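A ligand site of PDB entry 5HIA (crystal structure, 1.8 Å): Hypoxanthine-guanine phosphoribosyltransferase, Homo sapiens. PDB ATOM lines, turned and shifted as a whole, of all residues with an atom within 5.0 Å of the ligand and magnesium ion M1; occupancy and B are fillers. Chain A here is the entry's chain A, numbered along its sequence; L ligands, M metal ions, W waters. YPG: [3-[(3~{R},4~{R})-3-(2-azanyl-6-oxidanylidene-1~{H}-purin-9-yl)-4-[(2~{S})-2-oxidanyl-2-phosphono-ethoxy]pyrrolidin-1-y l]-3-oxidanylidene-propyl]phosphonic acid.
Magnesium ion M1 is bound by the side-chain carboxylate of Asp 200 (2.0 Å), water W2 (2.2 Å), an oxygen (OAB) of the ligand (2.2 Å), an oxygen (OAD) of the ligand (2.2 Å), water W4 (2.2 Å) and water W6 (2.3 Å).
OD2 of Asp 200 is in salt-bridge range of NH2 of Arg 206, at 3.4 Å.
OG1 of Thr 145 lies within hydrogen-bond range of N of Lys 147 (3.3 Å).
O of Lys 192 is in hydrogen-bond range of NZ of Lys 172 (3.1 Å).
The backbone NH of Lys 172 sits at hydrogen-bond distance from the backbone carbonyl oxygen of Ile 143 (2.9 Å).
Arg 206 touches magnesium ion M1.
Of the 26 residues printed, 2 come within 4 Å of magnesium ion M1.
The nearest printed residue that does not touch magnesium ion M1 is Tyr 201 (5.6 Å).
Water W3 bridges the side-chain carboxylate of Asp 141 (2.7 Å) and an oxygen (OAH) of the ligand (2.7 Å).
Water W11 lies within hydrogen-bond range of OAG of the ligand (2.7 Å), NH2 of Arg 107 (3.0 Å) and NH2 of Arg 206 (3.4 Å).
Water W8 lies within hydrogen-bond range of an oxygen (OAH) of the ligand (2.7 Å), the backbone carbonyl oxygen of Val 73 (2.9 Å) and the backbone NH of Gly 76 (3.4 Å).
Water W1 lies within hydrogen-bond range of the guanidinium group (NE) of Arg 107 (2.6 Å), an oxygen (OAG) of the ligand (2.8 Å) and the backbone carbonyl oxygen (O) of Leu 108 (3.2 Å).
Water W10 lies within hydrogen-bond range of OE2 of Glu 140 (2.8 Å), OAF of the ligand (2.9 Å) and O of Ile 142 (2.9 Å).
Water W7 bridges the backbone carbonyl oxygen of Ile 142 (2.5 Å) and an oxygen (OAT) of the ligand (2.9 Å).
O6 of the ligand lies close to O of Lys 192 (3.4 Å).
Residues that only touch the ligand: Leu 74 (3.8 Å), Ile 142 (3.4 Å), Ile 143 (3.9 Å), Phe 193 (3.3 Å) and Leu 199 (3.5 Å).
Within 4 Å of the ligand: Leu 74, Lys 75, Gly 76, Ile 142, Ile 143, Asp 144, Thr 145, Gly 146, Lys 147, Thr 148, Lys 172, Lys 192, Phe 193, Val 194, Leu 199, Asp 200 and Arg 206.
The backbone carbonyl oxygen (O) of Asp 200 sits at hydrogen-bond distance from a nitrogen (N2) of the ligand (2.7 Å).
N of Thr 145 sits at hydrogen-bond distance from OAJ of the ligand, at 2.8 Å.
An oxygen (OAJ) of the ligand sits at hydrogen-bond distance from the side-chain hydroxyl of Thr 145 (2.5 Å).
N of Val 194 sits at hydrogen-bond distance from O6 of the ligand (3.1 Å).
O of Val 194 is in hydrogen-bond range of N1 of the ligand, 2.6 Å away.
The backbone NH (N) of Thr 148 sits at hydrogen-bond distance from an oxygen (OAI) of the ligand, 2.7 Å away.
The side-chain hydroxyl (OG1) of Thr 148 lies within hydrogen-bond range of an oxygen (OAI) of the ligand, 2.8 Å away.
NZ of Lys 172 sits at hydrogen-bond distance from O6 of the ligand, at 2.8 Å.
The backbone NH of Gly 146 sits at hydrogen-bond distance from an oxygen (OAE) of the ligand, at 2.8 Å.
The backbone NH of Lys 75 sits at hydrogen-bond distance from an oxygen (OAG) of the ligand (2.8 Å).
An oxygen (OAG) of the ligand is in salt-bridge range of the guanidinium group of Arg 206, at 3.4 Å.
An oxygen (OAE) of the ligand lies within hydrogen-bond range of the backbone NH (N) of Asp 144 (3.0 Å).
The backbone NH of Gly 76 lies within hydrogen-bond range of an oxygen (OAH) of the ligand, 3.0 Å away.
The backbone NH (N) of Lys 147 lies within hydrogen-bond range of an oxygen (OAI) of the ligand (3.4 Å).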
ATOM      1  N   VAL A  73      -5.115   2.745 -34.152  1.00  0.00           N
ATOM      2  CA  VAL A  73      -4.741   2.551 -32.748  1.00  0.00           C
ATOM      3  C   VAL A  73      -4.039   1.208 -32.553  1.00  0.00           C
ATOM      4  O   VAL A  73      -4.658   0.140 -32.616  1.00  0.00           O
ATOM      5  CB  VAL A  73      -5.962   2.648 -31.791  1.00  0.00           C
ATOM      6  CG1 VAL A  73      -5.492   2.586 -30.357  1.00  0.00           C
ATOM      7  CG2 VAL A  73      -6.732   3.916 -32.038  1.00  0.00           C
ATOM      8  N   LEU A  74      -2.731   1.279 -32.348  1.00  0.00           N
ATOM      9  CA  LEU A  74      -1.863   0.109 -32.238  1.00  0.00           C
ATOM     10  C   LEU A  74      -1.941  -0.477 -30.834  1.00  0.00           C
ATOM     11  O   LEU A  74      -2.214   0.255 -29.881  1.00  0.00           O
ATOM     12  CB  LEU A  74      -0.414   0.505 -32.558  1.00  0.00           C
ATOM     13  CG  LEU A  74      -0.130   0.864 -34.022  1.00  0.00           C
ATOM     14  CD1 LEU A  74       1.268   1.456 -34.189  1.00  0.00           C
ATOM     15  CD2 LEU A  74      -0.309  -0.356 -34.893  1.00  0.00           C
ATOM     16  N   LYS A  75      -1.673  -1.783 -30.676  1.00  0.00           N
ATOM     17  CA  LYS A  75      -1.313  -2.693 -31.769  1.00  0.00           C
ATOM     18  C   LYS A  75      -2.530  -3.348 -32.411  1.00  0.00           C
ATOM     19  O   LYS A  75      -2.514  -3.664 -33.594  1.00  0.00           O
ATOM     20  CB  LYS A  75      -0.383  -3.814 -31.274  1.00  0.00           C
ATOM     21  CG  LYS A  75       1.043  -3.415 -30.871  1.00  0.00           C
ATOM     22  CD  LYS A  75       1.768  -4.662 -30.373  1.00  0.00           C
ATOM     23  CE  LYS A  75       3.127  -4.397 -29.794  1.00  0.00           C
ATOM     24  NZ  LYS A  75       3.700  -5.657 -29.246  1.00  0.00           N
ATOM     25  N   GLY A  76      -3.562  -3.552 -31.598  1.00  0.00           N
ATOM     26  CA  GLY A  76      -4.711  -4.355 -31.987  1.00  0.00           C
ATOM     27  C   GLY A  76      -5.459  -3.876 -33.217  1.00  0.00           C
ATOM     28  O   GLY A  76      -6.050  -4.675 -33.934  1.00  0.00           O
ATOM     29  N   GLY A  77      -5.428  -2.572 -33.468  1.00  0.00           N
ATOM     30  CA  GLY A  77      -6.163  -2.050 -34.597  1.00  0.00           C
ATOM     31  C   GLY A  77      -5.544  -2.297 -35.960  1.00  0.00           C
ATOM     32  O   GLY A  77      -6.202  -2.047 -36.961  1.00  0.00           O
ATOM     33  N   ARG A 107      -0.167   4.690 -30.398  1.00  0.00           N
ATOM     34  CA  ARG A 107      -0.242   3.532 -29.518  1.00  0.00           C
ATOM     35  C   ARG A 107      -0.549   3.944 -28.098  1.00  0.00           C
ATOM     36  O   ARG A 107       0.074   4.859 -27.570  1.00  0.00           O
ATOM     37  CB  ARG A 107       1.060   2.739 -29.564  1.00  0.00           C
ATOM     38  CG  ARG A 107       1.087   1.592 -28.574  1.00  0.00           C
ATOM     39  CD  ARG A 107       2.223   0.615 -28.837  1.00  0.00           C
ATOM     40  NE  ARG A 107       2.114  -0.555 -27.985  1.00  0.00           N
ATOM     41  CZ  ARG A 107       3.129  -1.312 -27.612  1.00  0.00           C
ATOM     42  NH1 ARG A 107       4.353  -1.016 -28.017  1.00  0.00           N
ATOM     43  NH2 ARG A 107       2.936  -2.369 -26.836  1.00  0.00           N
ATOM     44  N   LEU A 108      -1.508   3.272 -27.470  1.00  0.00           N
ATOM     45  CA  LEU A 108      -1.855   3.534 -26.079  1.00  0.00           C
ATOM     46  C   LEU A 108      -1.636   2.291 -25.227  1.00  0.00           C
ATOM     47  O   LEU A 108      -1.971   1.175 -25.637  1.00  0.00           O
ATOM     48  CB  LEU A 108      -3.314   4.000 -25.949  1.00  0.00           C
ATOM     49  CG  LEU A 108      -3.670   5.453 -26.254  1.00  0.00           C
ATOM     50  CD1 LEU A 108      -3.392   5.855 -27.685  1.00  0.00           C
ATOM     51  CD2 LEU A 108      -5.137   5.689 -25.926  1.00  0.00           C
ATOM     52  N   GLU A 140     -10.148   1.289 -34.396  1.00  0.00           N
ATOM     53  CA  GLU A 140      -9.896   0.502 -33.203  1.00  0.00           C
ATOM     54  C   GLU A 140     -10.295  -0.975 -33.399  1.00  0.00           C
ATOM     55  O   GLU A 140     -11.140  -1.276 -34.238  1.00  0.00           O
ATOM     56  CB  GLU A 140     -10.684   1.123 -32.033  1.00  0.00           C
ATOM     57  CG  GLU A 140     -10.459   0.524 -30.659  1.00  0.00           C
ATOM     58  CD  GLU A 140      -9.071   0.765 -30.105  1.00  0.00           C
ATOM     59  OE1 GLU A 140      -8.171   0.006 -30.486  1.00  0.00           O
ATOM     60  OE2 GLU A 140      -8.862   1.668 -29.261  1.00  0.00           O
ATOM     61  N   ASP A 141      -9.686  -1.880 -32.635  1.00  0.00           N
ATOM     62  CA  ASP A 141     -10.081  -3.296 -32.670  1.00  0.00           C
ATOM     63  C   ASP A 141     -11.329  -3.525 -31.827  1.00  0.00           C
ATOM     64  O   ASP A 141     -12.295  -4.175 -32.263  1.00  0.00           O
ATOM     65  CB  ASP A 141      -8.932  -4.193 -32.186  1.00  0.00           C
ATOM     66  CG  ASP A 141      -8.387  -3.770 -30.819  1.00  0.00           C
ATOM     67  OD1 ASP A 141      -8.583  -2.608 -30.418  1.00  0.00           O
ATOM     68  OD2 ASP A 141      -7.738  -4.593 -30.137  1.00  0.00           O
ATOM     69  N   ILE A 142     -11.346  -2.978 -30.614  1.00  0.00           N
ATOM     70  CA  ILE A 142     -12.453  -3.280 -29.732  1.00  0.00           C
ATOM     71  C   ILE A 142     -12.711  -2.180 -28.694  1.00  0.00           C
ATOM     72  O   ILE A 142     -11.786  -1.575 -28.139  1.00  0.00           O
ATOM     73  CB  ILE A 142     -12.244  -4.652 -29.015  1.00  0.00           C
ATOM     74  CG1 ILE A 142     -13.502  -5.042 -28.228  1.00  0.00           C
ATOM     75  CG2 ILE A 142     -10.998  -4.629 -28.128  1.00  0.00           C
ATOM     76  CD1 ILE A 142     -13.492  -6.481 -27.719  1.00  0.00           C
ATOM     77  N   ILE A 143     -13.995  -1.926 -28.481  1.00  0.00           N
ATOM     78  CA  ILE A 143     -14.460  -1.056 -27.412  1.00  0.00           C
ATOM     79  C   ILE A 143     -15.078  -1.928 -26.332  1.00  0.00           C
ATOM     80  O   ILE A 143     -15.959  -2.745 -26.607  1.00  0.00           O
ATOM     81  CB  ILE A 143     -15.457  -0.036 -27.938  1.00  0.00           C
ATOM     82  CG1 ILE A 143     -14.749   0.824 -28.977  1.00  0.00           C
ATOM     83  CG2 ILE A 143     -16.082   0.769 -26.787  1.00  0.00           C
ATOM     84  CD1 ILE A 143     -15.498   2.033 -29.384  1.00  0.00           C
ATOM     85  N   ASP A 144     -14.577  -1.783 -25.113  1.00  0.00           N
ATOM     86  CA  ASP A 144     -15.053  -2.543 -23.975  1.00  0.00           C
ATOM     87  C   ASP A 144     -15.703  -1.557 -23.003  1.00  0.00           C
ATOM     88  O   ASP A 144     -16.902  -1.303 -23.095  1.00  0.00           O
ATOM     89  CB  ASP A 144     -13.908  -3.334 -23.335  1.00  0.00           C
ATOM     90  CG  ASP A 144     -14.342  -4.171 -22.128  1.00  0.00           C
ATOM     91  OD1 ASP A 144     -15.541  -4.463 -21.980  1.00  0.00           O
ATOM     92  OD2 ASP A 144     -13.463  -4.531 -21.317  1.00  0.00           O
ATOM     93  N   THR A 145     -14.916  -0.972 -22.097  1.00  0.00           N
ATOM     94  CA  THR A 145     -15.478   0.009 -21.181  1.00  0.00           C
ATOM     95  C   THR A 145     -15.761   1.315 -21.909  1.00  0.00           C
ATOM     96  O   THR A 145     -16.712   2.025 -21.578  1.00  0.00           O
ATOM     97  CB  THR A 145     -14.543   0.294 -19.961  1.00  0.00           C
ATOM     98  OG1 THR A 145     -13.276   0.786 -20.418  1.00  0.00           O
ATOM     99  CG2 THR A 145     -14.342  -0.965 -19.138  1.00  0.00           C
ATOM    100  N   GLY A 146     -14.946   1.617 -22.926  1.00  0.00           N
ATOM    101  CA  GLY A 146     -15.048   2.875 -23.637  1.00  0.00           C
ATOM    102  C   GLY A 146     -14.108   3.969 -23.100  1.00  0.00           C
ATOM    103  O   GLY A 146     -13.940   5.017 -23.735  1.00  0.00           O
ATOM    104  N   LYS A 147     -13.475   3.711 -21.958  1.00  0.00           N
ATOM    105  CA  LYS A 147     -12.637   4.737 -21.342  1.00  0.00           C
ATOM    106  C   LYS A 147     -11.443   5.140 -22.214  1.00  0.00           C
ATOM    107  O   LYS A 147     -11.050   6.315 -22.221  1.00  0.00           O
ATOM    108  CB  LYS A 147     -12.168   4.278 -19.966  1.00  0.00           C
ATOM    109  CG  LYS A 147     -13.302   4.160 -18.974  1.00  0.00           C
ATOM    110  CD  LYS A 147     -12.835   3.623 -17.637  1.00  0.00           C
ATOM    111  CE  LYS A 147     -14.008   3.454 -16.687  1.00  0.00           C
ATOM    112  NZ  LYS A 147     -13.543   3.019 -15.355  1.00  0.00           N
ATOM    113  N   THR A 148     -10.871   4.186 -22.944  1.00  0.00           N
ATOM    114  CA  THR A 148      -9.728   4.490 -23.818  1.00  0.00           C
ATOM    115  C   THR A 148     -10.135   5.436 -24.939  1.00  0.00           C
ATOM    116  O   THR A 148      -9.442   6.431 -25.202  1.00  0.00           O
ATOM    117  CB  THR A 148      -9.131   3.226 -24.451  1.00  0.00           C
ATOM    118  OG1 THR A 148      -8.564   2.400 -23.427  1.00  0.00           O
ATOM    119  CG2 THR A 148      -8.042   3.579 -25.449  1.00  0.00           C
ATOM    120  N   MET A 149     -11.263   5.148 -25.596  1.00  0.00           N
ATOM    121  CA  MET A 149     -11.721   5.985 -26.693  1.00  0.00           C
ATOM    122  C   MET A 149     -12.117   7.383 -26.243  1.00  0.00           C
ATOM    123  O   MET A 149     -11.848   8.355 -26.954  1.00  0.00           O
ATOM    124  CB  MET A 149     -12.891   5.337 -27.416  1.00  0.00           C
ATOM    125  CG  MET A 149     -13.105   5.886 -28.818  1.00  0.00           C
ATOM    126  SD  MET A 149     -11.598   6.160 -29.788  1.00  0.00           S
ATOM    127  CE  MET A 149     -10.913   4.517 -29.849  1.00  0.00           C
ATOM    128  N   LYS A 172     -18.152  -4.583 -27.243  1.00  0.00           N
ATOM    129  CA  LYS A 172     -18.534  -5.585 -26.269  1.00  0.00           C
ATOM    130  C   LYS A 172     -19.744  -5.135 -25.424  1.00  0.00           C
ATOM    131  O   LYS A 172     -19.788  -3.992 -24.947  1.00  0.00           O
ATOM    132  CB  LYS A 172     -17.311  -5.891 -25.376  1.00  0.00           C
ATOM    133  CG  LYS A 172     -17.453  -7.116 -24.492  1.00  0.00           C
ATOM    134  CD  LYS A 172     -16.154  -7.400 -23.728  1.00  0.00           C
ATOM    135  CE  LYS A 172     -15.175  -8.244 -24.546  1.00  0.00           C
ATOM    136  NZ  LYS A 172     -14.059  -8.761 -23.691  1.00  0.00           N
ATOM    137  N   LYS A 192     -17.183 -11.795 -23.519  1.00  0.00           N
ATOM    138  CA  LYS A 192     -16.296 -12.942 -23.651  1.00  0.00           C
ATOM    139  C   LYS A 192     -14.948 -12.427 -24.129  1.00  0.00           C
ATOM    140  O   LYS A 192     -14.897 -11.474 -24.908  1.00  0.00           O
ATOM    141  CB  LYS A 192     -16.822 -13.978 -24.668  1.00  0.00           C
ATOM    142  CG  LYS A 192     -18.036 -14.767 -24.230  1.00  0.00           C
ATOM    143  CD  LYS A 192     -18.266 -15.889 -25.237  1.00  0.00           C
ATOM    144  CE  LYS A 192     -19.408 -16.806 -24.820  1.00  0.00           C
ATOM    145  NZ  LYS A 192     -19.629 -17.841 -25.868  1.00  0.00           N
ATOM    146  N   PHE A 193     -13.863 -13.049 -23.696  1.00  0.00           N
ATOM    147  CA  PHE A 193     -12.537 -12.638 -24.170  1.00  0.00           C
ATOM    148  C   PHE A 193     -12.226 -13.314 -25.505  1.00  0.00           C
ATOM    149  O   PHE A 193     -12.195 -14.546 -25.590  1.00  0.00           O
ATOM    150  CB  PHE A 193     -11.456 -12.969 -23.150  1.00  0.00           C
ATOM    151  CG  PHE A 193     -10.136 -12.306 -23.425  1.00  0.00           C
ATOM    152  CD1 PHE A 193      -9.847 -11.073 -22.884  1.00  0.00           C
ATOM    153  CD2 PHE A 193      -9.185 -12.930 -24.224  1.00  0.00           C
ATOM    154  CE1 PHE A 193      -8.639 -10.448 -23.129  1.00  0.00           C
ATOM    155  CE2 PHE A 193      -7.970 -12.329 -24.471  1.00  0.00           C
ATOM    156  CZ  PHE A 193      -7.686 -11.088 -23.934  1.00  0.00           C
ATOM    157  N   VAL A 194     -11.998 -12.509 -26.533  1.00  0.00           N
ATOM    158  CA  VAL A 194     -11.768 -13.039 -27.870  1.00  0.00           C
ATOM    159  C   VAL A 194     -10.358 -12.661 -28.312  1.00  0.00           C
ATOM    160  O   VAL A 194      -9.785 -11.689 -27.815  1.00  0.00           O
ATOM    161  CB  VAL A 194     -12.808 -12.518 -28.884  1.00  0.00           C
ATOM    162  CG1 VAL A 194     -14.198 -13.021 -28.514  1.00  0.00           C
ATOM    163  CG2 VAL A 194     -12.769 -10.999 -28.966  1.00  0.00           C
ATOM    164  N   VAL A 195      -9.808 -13.445 -29.241  1.00  0.00           N
ATOM    165  CA  VAL A 195      -8.473 -13.213 -29.779  1.00  0.00           C
ATOM    166  C   VAL A 195      -8.482 -13.402 -31.291  1.00  0.00           C
ATOM    167  O   VAL A 195      -9.466 -13.896 -31.825  1.00  0.00           O
ATOM    168  CB  VAL A 195      -7.410 -14.158 -29.154  1.00  0.00           C
ATOM    169  CG1 VAL A 195      -7.219 -13.852 -27.679  1.00  0.00           C
ATOM    170  CG2 VAL A 195      -7.761 -15.619 -29.375  1.00  0.00           C
ATOM    171  N   LEU A 199      -6.139  -9.101 -32.418  1.00  0.00           N
ATOM    172  CA  LEU A 199      -6.457  -9.051 -30.989  1.00  0.00           C
ATOM    173  C   LEU A 199      -5.640 -10.092 -30.227  1.00  0.00           C
ATOM    174  O   LEU A 199      -5.658 -11.275 -30.574  1.00  0.00           O
ATOM    175  CB  LEU A 199      -7.956  -9.260 -30.746  1.00  0.00           C
ATOM    176  CG  LEU A 199      -8.766  -8.005 -31.082  1.00  0.00           C
ATOM    177  CD1 LEU A 199      -9.299  -8.017 -32.507  1.00  0.00           C
ATOM    178  CD2 LEU A 199      -9.885  -7.811 -30.072  1.00  0.00           C
ATOM    179  N   ASP A 200      -4.940  -9.665 -29.186  1.00  0.00           N
ATOM    180  CA  ASP A 200      -3.999 -10.557 -28.524  1.00  0.00           C
ATOM    181  C   ASP A 200      -4.398 -11.008 -27.134  1.00  0.00           C
ATOM    182  O   ASP A 200      -5.243 -10.417 -26.455  1.00  0.00           O
ATOM    183  CB  ASP A 200      -2.627  -9.900 -28.407  1.00  0.00           C
ATOM    184  CG  ASP A 200      -2.590  -8.862 -27.295  1.00  0.00           C
ATOM    185  OD1 ASP A 200      -3.400  -7.933 -27.380  1.00  0.00           O
ATOM    186  OD2 ASP A 200      -1.779  -8.983 -26.350  1.00  0.00           O
ATOM    187  N   TYR A 201      -3.727 -12.066 -26.705  1.00  0.00           N
ATOM    188  CA  TYR A 201      -3.687 -12.435 -25.307  1.00  0.00           C
ATOM    189  C   TYR A 201      -2.214 -12.522 -24.922  1.00  0.00           C
ATOM    190  O   TYR A 201      -1.512 -13.455 -25.318  1.00  0.00           O
ATOM    191  CB  TYR A 201      -4.431 -13.755 -25.090  1.00  0.00           C
ATOM    192  CG  TYR A 201      -4.277 -14.308 -23.697  1.00  0.00           C
ATOM    193  CD1 TYR A 201      -4.862 -13.674 -22.606  1.00  0.00           C
ATOM    194  CD2 TYR A 201      -3.550 -15.468 -23.468  1.00  0.00           C
ATOM    195  CE1 TYR A 201      -4.720 -14.185 -21.326  1.00  0.00           C
ATOM    196  CE2 TYR A 201      -3.412 -15.986 -22.198  1.00  0.00           C
ATOM    197  CZ  TYR A 201      -3.994 -15.328 -21.136  1.00  0.00           C
ATOM    198  OH  TYR A 201      -3.860 -15.840 -19.871  1.00  0.00           O
ATOM    199  N   ARG A 206      -2.097 -12.735 -32.332  1.00  0.00           N
ATOM    200  CA  ARG A 206      -2.220 -11.679 -33.328  1.00  0.00           C
ATOM    201  C   ARG A 206      -2.076 -12.274 -34.729  1.00  0.00           C
ATOM    202  O   ARG A 206      -2.709 -11.817 -35.678  1.00  0.00           O
ATOM    203  CB  ARG A 206      -1.183 -10.580 -33.102  1.00  0.00           C
ATOM    204  CG  ARG A 206      -1.385  -9.839 -31.773  1.00  0.00           C
ATOM    205  CD  ARG A 206      -0.844  -8.412 -31.848  1.00  0.00           C
ATOM    206  NE  ARG A 206      -0.556  -7.831 -30.547  1.00  0.00           N
ATOM    207  CZ  ARG A 206      -1.393  -7.073 -29.862  1.00  0.00           C
ATOM    208  NH1 ARG A 206      -2.592  -6.789 -30.360  1.00  0.00           N
ATOM    209  NH2 ARG A 206      -1.027  -6.571 -28.683  1.00  0.00           N
HETATM  210  C4  YPG L   1      -9.597  -6.995 -25.285  1.00  0.00           C
HETATM  211  C5  YPG L   1     -10.795  -7.630 -25.090  1.00  0.00           C
HETATM  212  C6  YPG L   1     -10.986  -8.957 -25.646  1.00  0.00           C
HETATM  213  C8  YPG L   1     -10.931  -5.611 -24.091  1.00  0.00           C
HETATM  214  N1  YPG L   1      -9.932  -9.510 -26.326  1.00  0.00           N
HETATM  215  N2  YPG L   1      -7.714  -9.531 -27.249  1.00  0.00           N
HETATM  216  N3  YPG L   1      -8.561  -7.639 -26.008  1.00  0.00           N
HETATM  217  OAI YPG L   1     -11.078   1.495 -22.733  1.00  0.00           O
HETATM  218  PBF YPG L   1     -11.645   0.078 -23.224  1.00  0.00           P
HETATM  219  OAJ YPG L   1     -12.081  -0.779 -22.002  1.00  0.00           O
HETATM  220  OAE YPG L   1     -12.801   0.391 -24.175  1.00  0.00           O
HETATM  221  CAZ YPG L   1     -10.293  -0.786 -24.067  1.00  0.00           C
HETATM  222  OAF YPG L   1      -9.639   0.109 -24.863  1.00  0.00           O
HETATM  223  CAN YPG L   1     -10.805  -1.957 -24.864  1.00  0.00           C
HETATM  224  OAT YPG L   1      -9.791  -2.869 -25.329  1.00  0.00           O
HETATM  225  CBA YPG L   1      -8.873  -3.371 -24.398  1.00  0.00           C
HETATM  226  CAO YPG L   1      -7.542  -2.809 -24.653  1.00  0.00           C
HETATM  227  NBC YPG L   1      -6.603  -3.921 -24.542  1.00  0.00           N
HETATM  228  CAU YPG L   1      -5.217  -3.878 -24.920  1.00  0.00           C
HETATM  229  OAB YPG L   1      -4.532  -4.890 -24.776  1.00  0.00           O
HETATM  230  CAL YPG L   1      -4.622  -2.594 -25.455  1.00  0.00           C
HETATM  231  CAM YPG L   1      -3.204  -2.690 -26.070  1.00  0.00           C
HETATM  232  PBE YPG L   1      -3.058  -3.544 -27.763  1.00  0.00           P
HETATM  233  OAG YPG L   1      -1.559  -3.252 -28.262  1.00  0.00           O
HETATM  234  OAH YPG L   1      -4.077  -2.884 -28.744  1.00  0.00           O
HETATM  235  OAD YPG L   1      -3.300  -5.036 -27.623  1.00  0.00           O
HETATM  236  CAP YPG L   1      -7.277  -5.064 -24.042  1.00  0.00           C
HETATM  237  CBB YPG L   1      -8.611  -4.779 -24.661  1.00  0.00           C
HETATM  238  N9  YPG L   1      -9.693  -5.737 -24.656  1.00  0.00           N
HETATM  239  C2  YPG L   1      -8.755  -8.885 -26.517  1.00  0.00           C
HETATM  240  O6  YPG L   1     -12.153  -9.632 -25.483  1.00  0.00           O
HETATM  241  N7  YPG L   1     -11.635  -6.750 -24.334  1.00  0.00           N
HETATM  242 MG    MG M   1      -3.940  -6.464 -26.126  1.00  0.00          MG
HETATM  243 MG    MG M   2      -7.538  -1.456 -29.114  1.00  0.00          MG
HETATM  244  O   HOH W   1      -0.274  -1.013 -27.213  1.00  0.00           O
HETATM  245  O   HOH W   2      -5.916  -6.506 -26.985  1.00  0.00           O
HETATM  246  O   HOH W   3      -6.729  -2.952 -28.280  1.00  0.00           O
HETATM  247  O   HOH W   4      -5.143  -7.897 -24.947  1.00  0.00           O
HETATM  248  O   HOH W   5      -5.489  -6.222 -29.522  1.00  0.00           O
HETATM  249  O   HOH W   6      -2.033  -6.743 -24.936  1.00  0.00           O
HETATM  250  O   HOH W   7      -9.318  -1.543 -27.863  1.00  0.00           O
HETATM  251  O   HOH W   8      -5.619  -1.216 -30.236  1.00  0.00           O
HETATM  252  O   HOH W   9     -12.498   2.501 -25.713  1.00  0.00           O
HETATM  253  O   HOH W  10     -10.813   1.052 -27.329  1.00  0.00           O
HETATM  254  O   HOH W  11       0.481  -4.161 -26.737  1.00  0.00           O
